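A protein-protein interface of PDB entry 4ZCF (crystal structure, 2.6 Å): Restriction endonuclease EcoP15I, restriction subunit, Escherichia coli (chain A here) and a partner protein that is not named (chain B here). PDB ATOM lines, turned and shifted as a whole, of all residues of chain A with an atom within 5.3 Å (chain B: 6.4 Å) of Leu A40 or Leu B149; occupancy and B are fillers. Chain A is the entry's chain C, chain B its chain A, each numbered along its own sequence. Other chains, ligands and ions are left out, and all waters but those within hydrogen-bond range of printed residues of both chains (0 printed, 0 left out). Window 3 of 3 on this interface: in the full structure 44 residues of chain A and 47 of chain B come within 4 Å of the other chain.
O of Leu A40 is in hydrogen-bond range of N of Asn A175, 2.8 Å away.
OG of Ser A174 lies within hydrogen-bond range of N of Phe A176 (3.2 Å).
Leu A40 touches three residues of chain B.
Leu B149 touches just these residues of chain A: Leu A40 and Phe A176.
Printed residues of chain A within 4 Å of Leu B72: Phe A176 (3.6 Å).
Printed residues of chain B within 4 Å of Ala A37: Gly B151.
Printed residues of chain B within 4 Å of Phe A176: Leu B68, Leu B72 and Leu B149.
Of the printed residues of chain A, Gly B151 touches Val A36 (3.6 Å), Ala A37 (3.8 Å) and Leu A40 (3.7 Å).
Gln B145 touches none of the printed residues of chain A.
The nearest residue of chain B that does not touch Leu A40 is Glu B148 (5.3 Å).
The nearest printed residue of chain A that does not touch Leu B149 is Ser A174 (6.4 Å).
Val A36 touches Gly B151.
Ala A37 touches Gly B151.
Leu B149 touches Leu A40.
Leu A40 touches Ala B150 (CD1 to O, 3.3 Å).
Gly B151 touches Leu A40 (CA to CD1, 3.7 Å).
Phe A176 touches Leu B68.
CD2 of Leu B72 touches CZ of Phe A176, 3.6 Å away.
Phe A176 touches Leu B149.
Of the 12 printed residues of chain A, 4 touch a printed residue of chain B.
Printed residues of chain A that touch a printed residue of chain B: Val A36, Ala A37, Leu A40 and Phe A176.
Hydrophobic or aromatic side chains of chain A that line the printed part of chain B: Val A36, Leu A40 and Phe A176.
Hydrophobic or aromatic side chains of chain B that line the printed part of chain A: Leu B68, Leu B72 and Leu B149.
Among the printed residues, 8 pairs touch across the chains.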
ATOM      1  N   VAL A  36       1.825  17.897  -5.364  1.00  0.00           N
ATOM      2  CA  VAL A  36       0.351  17.957  -5.407  1.00  0.00           C
ATOM      3  C   VAL A  36      -0.153  19.273  -6.016  1.00  0.00           C
ATOM      4  O   VAL A  36      -1.187  19.279  -6.690  1.00  0.00           O
ATOM      5  CB  VAL A  36      -0.305  17.672  -4.027  1.00  0.00           C
ATOM      6  CG1 VAL A  36      -1.709  17.101  -4.201  1.00  0.00           C
ATOM      7  CG2 VAL A  36       0.542  16.717  -3.193  1.00  0.00           C
ATOM      8  N   ALA A  37       0.586  20.376  -5.781  1.00  0.00           N
ATOM      9  CA  ALA A  37       0.265  21.700  -6.311  1.00  0.00           C
ATOM     10  C   ALA A  37       0.547  21.753  -7.818  1.00  0.00           C
ATOM     11  O   ALA A  37      -0.359  22.103  -8.580  1.00  0.00           O
ATOM     12  CB  ALA A  37       1.060  22.773  -5.579  1.00  0.00           C
ATOM     13  N   VAL A  38       1.779  21.353  -8.242  1.00  0.00           N
ATOM     14  CA  VAL A  38       2.228  21.318  -9.636  1.00  0.00           C
ATOM     15  C   VAL A  38       1.462  20.318 -10.519  1.00  0.00           C
ATOM     16  O   VAL A  38       1.349  20.544 -11.722  1.00  0.00           O
ATOM     17  CB  VAL A  38       3.721  21.043  -9.699  1.00  0.00           C
ATOM     18  N   ARG A  39       0.927  19.228  -9.931  1.00  0.00           N
ATOM     19  CA  ARG A  39       0.174  18.180 -10.639  1.00  0.00           C
ATOM     20  C   ARG A  39      -1.118  18.733 -11.270  1.00  0.00           C
ATOM     21  O   ARG A  39      -1.557  18.246 -12.321  1.00  0.00           O
ATOM     22  CB  ARG A  39      -0.133  17.011  -9.679  1.00  0.00           C
ATOM     23  CG  ARG A  39      -0.626  15.727 -10.355  1.00  0.00           C
ATOM     24  CD  ARG A  39      -0.222  14.476  -9.590  1.00  0.00           C
ATOM     25  NE  ARG A  39      -0.909  14.341  -8.302  1.00  0.00           N
ATOM     26  CZ  ARG A  39      -0.324  13.945  -7.176  1.00  0.00           C
ATOM     27  NH1 ARG A  39       0.969  13.644  -7.162  1.00  0.00           N
ATOM     28  NH2 ARG A  39      -1.026  13.852  -6.053  1.00  0.00           N
ATOM     29  N   LEU A  40      -1.703  19.745 -10.619  1.00  0.00           N
ATOM     30  CA  LEU A  40      -2.939  20.399 -11.029  1.00  0.00           C
ATOM     31  C   LEU A  40      -2.719  21.429 -12.157  1.00  0.00           C
ATOM     32  O   LEU A  40      -3.634  21.680 -12.941  1.00  0.00           O
ATOM     33  CB  LEU A  40      -3.597  21.058  -9.803  1.00  0.00           C
ATOM     34  CG  LEU A  40      -4.766  20.300  -9.175  1.00  0.00           C
ATOM     35  CD1 LEU A  40      -4.750  20.413  -7.681  1.00  0.00           C
ATOM     36  CD2 LEU A  40      -6.076  20.812  -9.682  1.00  0.00           C
ATOM     37  N   LEU A  41      -1.502  21.995 -12.249  1.00  0.00           N
ATOM     38  CA  LEU A  41      -1.158  23.018 -13.240  1.00  0.00           C
ATOM     39  C   LEU A  41      -0.291  22.490 -14.389  1.00  0.00           C
ATOM     40  O   LEU A  41      -0.357  23.026 -15.498  1.00  0.00           O
ATOM     41  CB  LEU A  41      -0.450  24.225 -12.567  1.00  0.00           C
ATOM     42  CG  LEU A  41      -1.015  24.785 -11.249  1.00  0.00           C
ATOM     43  CD1 LEU A  41       0.068  25.010 -10.282  1.00  0.00           C
ATOM     44  CD2 LEU A  41      -1.692  26.066 -11.458  1.00  0.00           C
ATOM     45  N   ALA A  42       0.579  21.509 -14.118  1.00  0.00           N
ATOM     46  CA  ALA A  42       1.476  20.992 -15.156  1.00  0.00           C
ATOM     47  C   ALA A  42       0.938  19.750 -15.850  1.00  0.00           C
ATOM     48  O   ALA A  42       0.038  19.089 -15.338  1.00  0.00           O
ATOM     49  CB  ALA A  42       2.880  20.745 -14.595  1.00  0.00           C
ATOM     50  N   LYS A 109      -2.430  20.751 -21.725  1.00  0.00           N
ATOM     51  CA  LYS A 109      -1.792  22.037 -21.970  1.00  0.00           C
ATOM     52  C   LYS A 109      -0.878  21.981 -23.186  1.00  0.00           C
ATOM     53  O   LYS A 109       0.065  21.189 -23.234  1.00  0.00           O
ATOM     54  CB  LYS A 109      -1.107  22.569 -20.700  1.00  0.00           C
ATOM     55  CG  LYS A 109      -2.122  23.188 -19.743  1.00  0.00           C
ATOM     56  CD  LYS A 109      -1.515  23.928 -18.596  1.00  0.00           C
ATOM     57  CE  LYS A 109      -2.600  24.200 -17.584  1.00  0.00           C
ATOM     58  NZ  LYS A 109      -2.066  24.925 -16.389  1.00  0.00           N
ATOM     59  N   ALA A 173      -4.134  27.968 -14.942  1.00  0.00           N
ATOM     60  CA  ALA A 173      -5.338  27.165 -15.212  1.00  0.00           C
ATOM     61  C   ALA A 173      -5.250  25.747 -14.648  1.00  0.00           C
ATOM     62  O   ALA A 173      -4.253  25.057 -14.844  1.00  0.00           O
ATOM     63  CB  ALA A 173      -5.612  27.120 -16.704  1.00  0.00           C
ATOM     64  N   SER A 174      -6.301  25.328 -13.934  1.00  0.00           N
ATOM     65  CA  SER A 174      -6.431  24.037 -13.244  1.00  0.00           C
ATOM     66  C   SER A 174      -6.788  22.869 -14.166  1.00  0.00           C
ATOM     67  O   SER A 174      -7.552  23.048 -15.117  1.00  0.00           O
ATOM     68  CB  SER A 174      -7.447  24.153 -12.107  1.00  0.00           C
ATOM     69  OG  SER A 174      -7.813  22.893 -11.568  1.00  0.00           O
ATOM     70  N   ASN A 175      -6.245  21.669 -13.846  1.00  0.00           N
ATOM     71  CA  ASN A 175      -6.456  20.398 -14.557  1.00  0.00           C
ATOM     72  C   ASN A 175      -7.705  19.673 -14.056  1.00  0.00           C
ATOM     73  O   ASN A 175      -8.286  18.898 -14.821  1.00  0.00           O
ATOM     74  CB  ASN A 175      -5.241  19.485 -14.399  1.00  0.00           C
ATOM     75  N   PHE A 176      -8.105  19.912 -12.780  1.00  0.00           N
ATOM     76  CA  PHE A 176      -9.275  19.319 -12.111  1.00  0.00           C
ATOM     77  C   PHE A 176     -10.415  18.986 -13.073  1.00  0.00           C
ATOM     78  O   PHE A 176     -11.015  17.919 -12.973  1.00  0.00           O
ATOM     79  CB  PHE A 176      -9.791  20.238 -10.984  1.00  0.00           C
ATOM     80  CG  PHE A 176     -11.035  19.732 -10.288  1.00  0.00           C
ATOM     81  CD1 PHE A 176     -10.939  18.890  -9.186  1.00  0.00           C
ATOM     82  CD2 PHE A 176     -12.304  20.082 -10.745  1.00  0.00           C
ATOM     83  CE1 PHE A 176     -12.090  18.399  -8.561  1.00  0.00           C
ATOM     84  CE2 PHE A 176     -13.451  19.579 -10.127  1.00  0.00           C
ATOM     85  CZ  PHE A 176     -13.337  18.746  -9.037  1.00  0.00           C
ATOM     86  N   LEU B  68     -11.166  25.853  -6.923  1.00  0.00           N
ATOM     87  CA  LEU B  68     -11.831  24.554  -7.009  1.00  0.00           C
ATOM     88  C   LEU B  68     -13.308  24.749  -7.383  1.00  0.00           C
ATOM     89  O   LEU B  68     -13.767  24.194  -8.388  1.00  0.00           O
ATOM     90  CB  LEU B  68     -11.707  23.833  -5.650  1.00  0.00           C
ATOM     91  CG  LEU B  68     -12.396  22.476  -5.522  1.00  0.00           C
ATOM     92  CD1 LEU B  68     -11.892  21.471  -6.589  1.00  0.00           C
ATOM     93  CD2 LEU B  68     -12.219  21.938  -4.150  1.00  0.00           C
ATOM     94  N   LEU B  72     -15.320  22.965 -10.451  1.00  0.00           N
ATOM     95  CA  LEU B  72     -16.297  21.952 -10.047  1.00  0.00           C
ATOM     96  C   LEU B  72     -17.439  21.983 -11.077  1.00  0.00           C
ATOM     97  O   LEU B  72     -17.838  23.076 -11.482  1.00  0.00           O
ATOM     98  CB  LEU B  72     -16.853  22.268  -8.639  1.00  0.00           C
ATOM     99  CG  LEU B  72     -16.131  21.635  -7.456  1.00  0.00           C
ATOM    100  CD1 LEU B  72     -16.675  22.142  -6.137  1.00  0.00           C
ATOM    101  CD2 LEU B  72     -16.220  20.138  -7.492  1.00  0.00           C
ATOM    102  N   PHE B 141     -17.649  19.418   2.354  1.00  0.00           N
ATOM    103  CA  PHE B 141     -16.574  18.427   2.238  1.00  0.00           C
ATOM    104  C   PHE B 141     -15.958  18.093   3.607  1.00  0.00           C
ATOM    105  O   PHE B 141     -16.226  18.777   4.601  1.00  0.00           O
ATOM    106  CB  PHE B 141     -15.454  18.903   1.278  1.00  0.00           C
ATOM    107  CG  PHE B 141     -15.820  19.233  -0.153  1.00  0.00           C
ATOM    108  CD1 PHE B 141     -16.174  18.229  -1.048  1.00  0.00           C
ATOM    109  CD2 PHE B 141     -15.719  20.535  -0.631  1.00  0.00           C
ATOM    110  CE1 PHE B 141     -16.489  18.532  -2.378  1.00  0.00           C
ATOM    111  CE2 PHE B 141     -16.030  20.836  -1.964  1.00  0.00           C
ATOM    112  CZ  PHE B 141     -16.416  19.835  -2.826  1.00  0.00           C
ATOM    113  N   GLU B 144     -10.249  15.635   4.509  1.00  0.00           N
ATOM    114  CA  GLU B 144      -9.594  14.601   3.704  1.00  0.00           C
ATOM    115  C   GLU B 144      -9.944  14.846   2.237  1.00  0.00           C
ATOM    116  O   GLU B 144      -9.039  14.967   1.407  1.00  0.00           O
ATOM    117  CB  GLU B 144     -10.005  13.167   4.158  1.00  0.00           C
ATOM    118  CG  GLU B 144     -10.497  13.014   5.599  1.00  0.00           C
ATOM    119  CD  GLU B 144      -9.542  13.333   6.742  1.00  0.00           C
ATOM    120  OE1 GLU B 144      -8.333  13.018   6.631  1.00  0.00           O
ATOM    121  OE2 GLU B 144     -10.019  13.860   7.774  1.00  0.00           O
ATOM    122  N   GLN B 145     -11.260  14.983   1.956  1.00  0.00           N
ATOM    123  CA  GLN B 145     -11.869  15.246   0.653  1.00  0.00           C
ATOM    124  C   GLN B 145     -11.328  16.525  -0.018  1.00  0.00           C
ATOM    125  O   GLN B 145     -10.916  16.472  -1.180  1.00  0.00           O
ATOM    126  CB  GLN B 145     -13.405  15.325   0.790  1.00  0.00           C
ATOM    127  CG  GLN B 145     -14.126  13.981   0.711  1.00  0.00           C
ATOM    128  CD  GLN B 145     -14.630  13.658  -0.679  1.00  0.00           C
ATOM    129  OE1 GLN B 145     -15.366  14.432  -1.309  1.00  0.00           O
ATOM    130  NE2 GLN B 145     -14.292  12.473  -1.166  1.00  0.00           N
ATOM    131  N   LEU B 146     -11.322  17.661   0.711  1.00  0.00           N
ATOM    132  CA  LEU B 146     -10.846  18.955   0.195  1.00  0.00           C
ATOM    133  C   LEU B 146      -9.343  18.964  -0.166  1.00  0.00           C
ATOM    134  O   LEU B 146      -8.978  19.449  -1.241  1.00  0.00           O
ATOM    135  CB  LEU B 146     -11.233  20.117   1.147  1.00  0.00           C
ATOM    136  CG  LEU B 146     -10.752  21.543   0.793  1.00  0.00           C
ATOM    137  CD1 LEU B 146     -11.255  21.989  -0.567  1.00  0.00           C
ATOM    138  CD2 LEU B 146     -11.169  22.535   1.859  1.00  0.00           C
ATOM    139  N   SER B 147      -8.498  18.401   0.726  1.00  0.00           N
ATOM    140  CA  SER B 147      -7.037  18.257   0.589  1.00  0.00           C
ATOM    141  C   SER B 147      -6.648  17.554  -0.716  1.00  0.00           C
ATOM    142  O   SER B 147      -5.686  17.965  -1.363  1.00  0.00           O
ATOM    143  CB  SER B 147      -6.485  17.478   1.779  1.00  0.00           C
ATOM    144  OG  SER B 147      -5.074  17.362   1.761  1.00  0.00           O
ATOM    145  N   GLU B 148      -7.420  16.513  -1.102  1.00  0.00           N
ATOM    146  CA  GLU B 148      -7.223  15.741  -2.325  1.00  0.00           C
ATOM    147  C   GLU B 148      -7.580  16.555  -3.586  1.00  0.00           C
ATOM    148  O   GLU B 148      -6.710  16.743  -4.440  1.00  0.00           O
ATOM    149  CB  GLU B 148      -8.036  14.455  -2.268  1.00  0.00           C
ATOM    150  N   LEU B 149      -8.842  17.057  -3.688  1.00  0.00           N
ATOM    151  CA  LEU B 149      -9.351  17.846  -4.828  1.00  0.00           C
ATOM    152  C   LEU B 149      -8.586  19.174  -5.054  1.00  0.00           C
ATOM    153  O   LEU B 149      -8.182  19.448  -6.183  1.00  0.00           O
ATOM    154  CB  LEU B 149     -10.861  18.138  -4.674  1.00  0.00           C
ATOM    155  CG  LEU B 149     -11.812  16.964  -4.443  1.00  0.00           C
ATOM    156  CD1 LEU B 149     -13.116  17.448  -3.868  1.00  0.00           C
ATOM    157  CD2 LEU B 149     -12.069  16.197  -5.713  1.00  0.00           C
ATOM    158  N   ALA B 150      -8.398  19.989  -3.990  1.00  0.00           N
ATOM    159  CA  ALA B 150      -7.684  21.270  -4.076  1.00  0.00           C
ATOM    160  C   ALA B 150      -6.184  21.128  -4.341  1.00  0.00           C
ATOM    161  O   ALA B 150      -5.583  22.035  -4.928  1.00  0.00           O
ATOM    162  CB  ALA B 150      -7.910  22.097  -2.821  1.00  0.00           C
ATOM    163  N   GLY B 151      -5.601  20.005  -3.907  1.00  0.00           N
ATOM    164  CA  GLY B 151      -4.176  19.736  -4.051  1.00  0.00           C
ATOM    165  C   GLY B 151      -3.346  20.538  -3.071  1.00  0.00           C
ATOM    166  O   GLY B 151      -2.359  21.178  -3.454  1.00  0.00           O
ATOM    167  N   ILE B 152      -3.762  20.516  -1.793  1.00  0.00           N
ATOM    168  CA  ILE B 152      -3.111  21.232  -0.698  1.00  0.00           C
ATOM    169  C   ILE B 152      -3.052  20.402   0.603  1.00  0.00           C
ATOM    170  O   ILE B 152      -3.875  19.506   0.781  1.00  0.00           O
ATOM    171  CB  ILE B 152      -3.719  22.663  -0.526  1.00  0.00           C
ATOM    172  CG1 ILE B 152      -2.776  23.613   0.288  1.00  0.00           C
ATOM    173  CG2 ILE B 152      -5.171  22.635   0.021  1.00  0.00           C
ATOM    174  CD1 ILE B 152      -1.162  23.687  -0.121  1.00  0.00           C
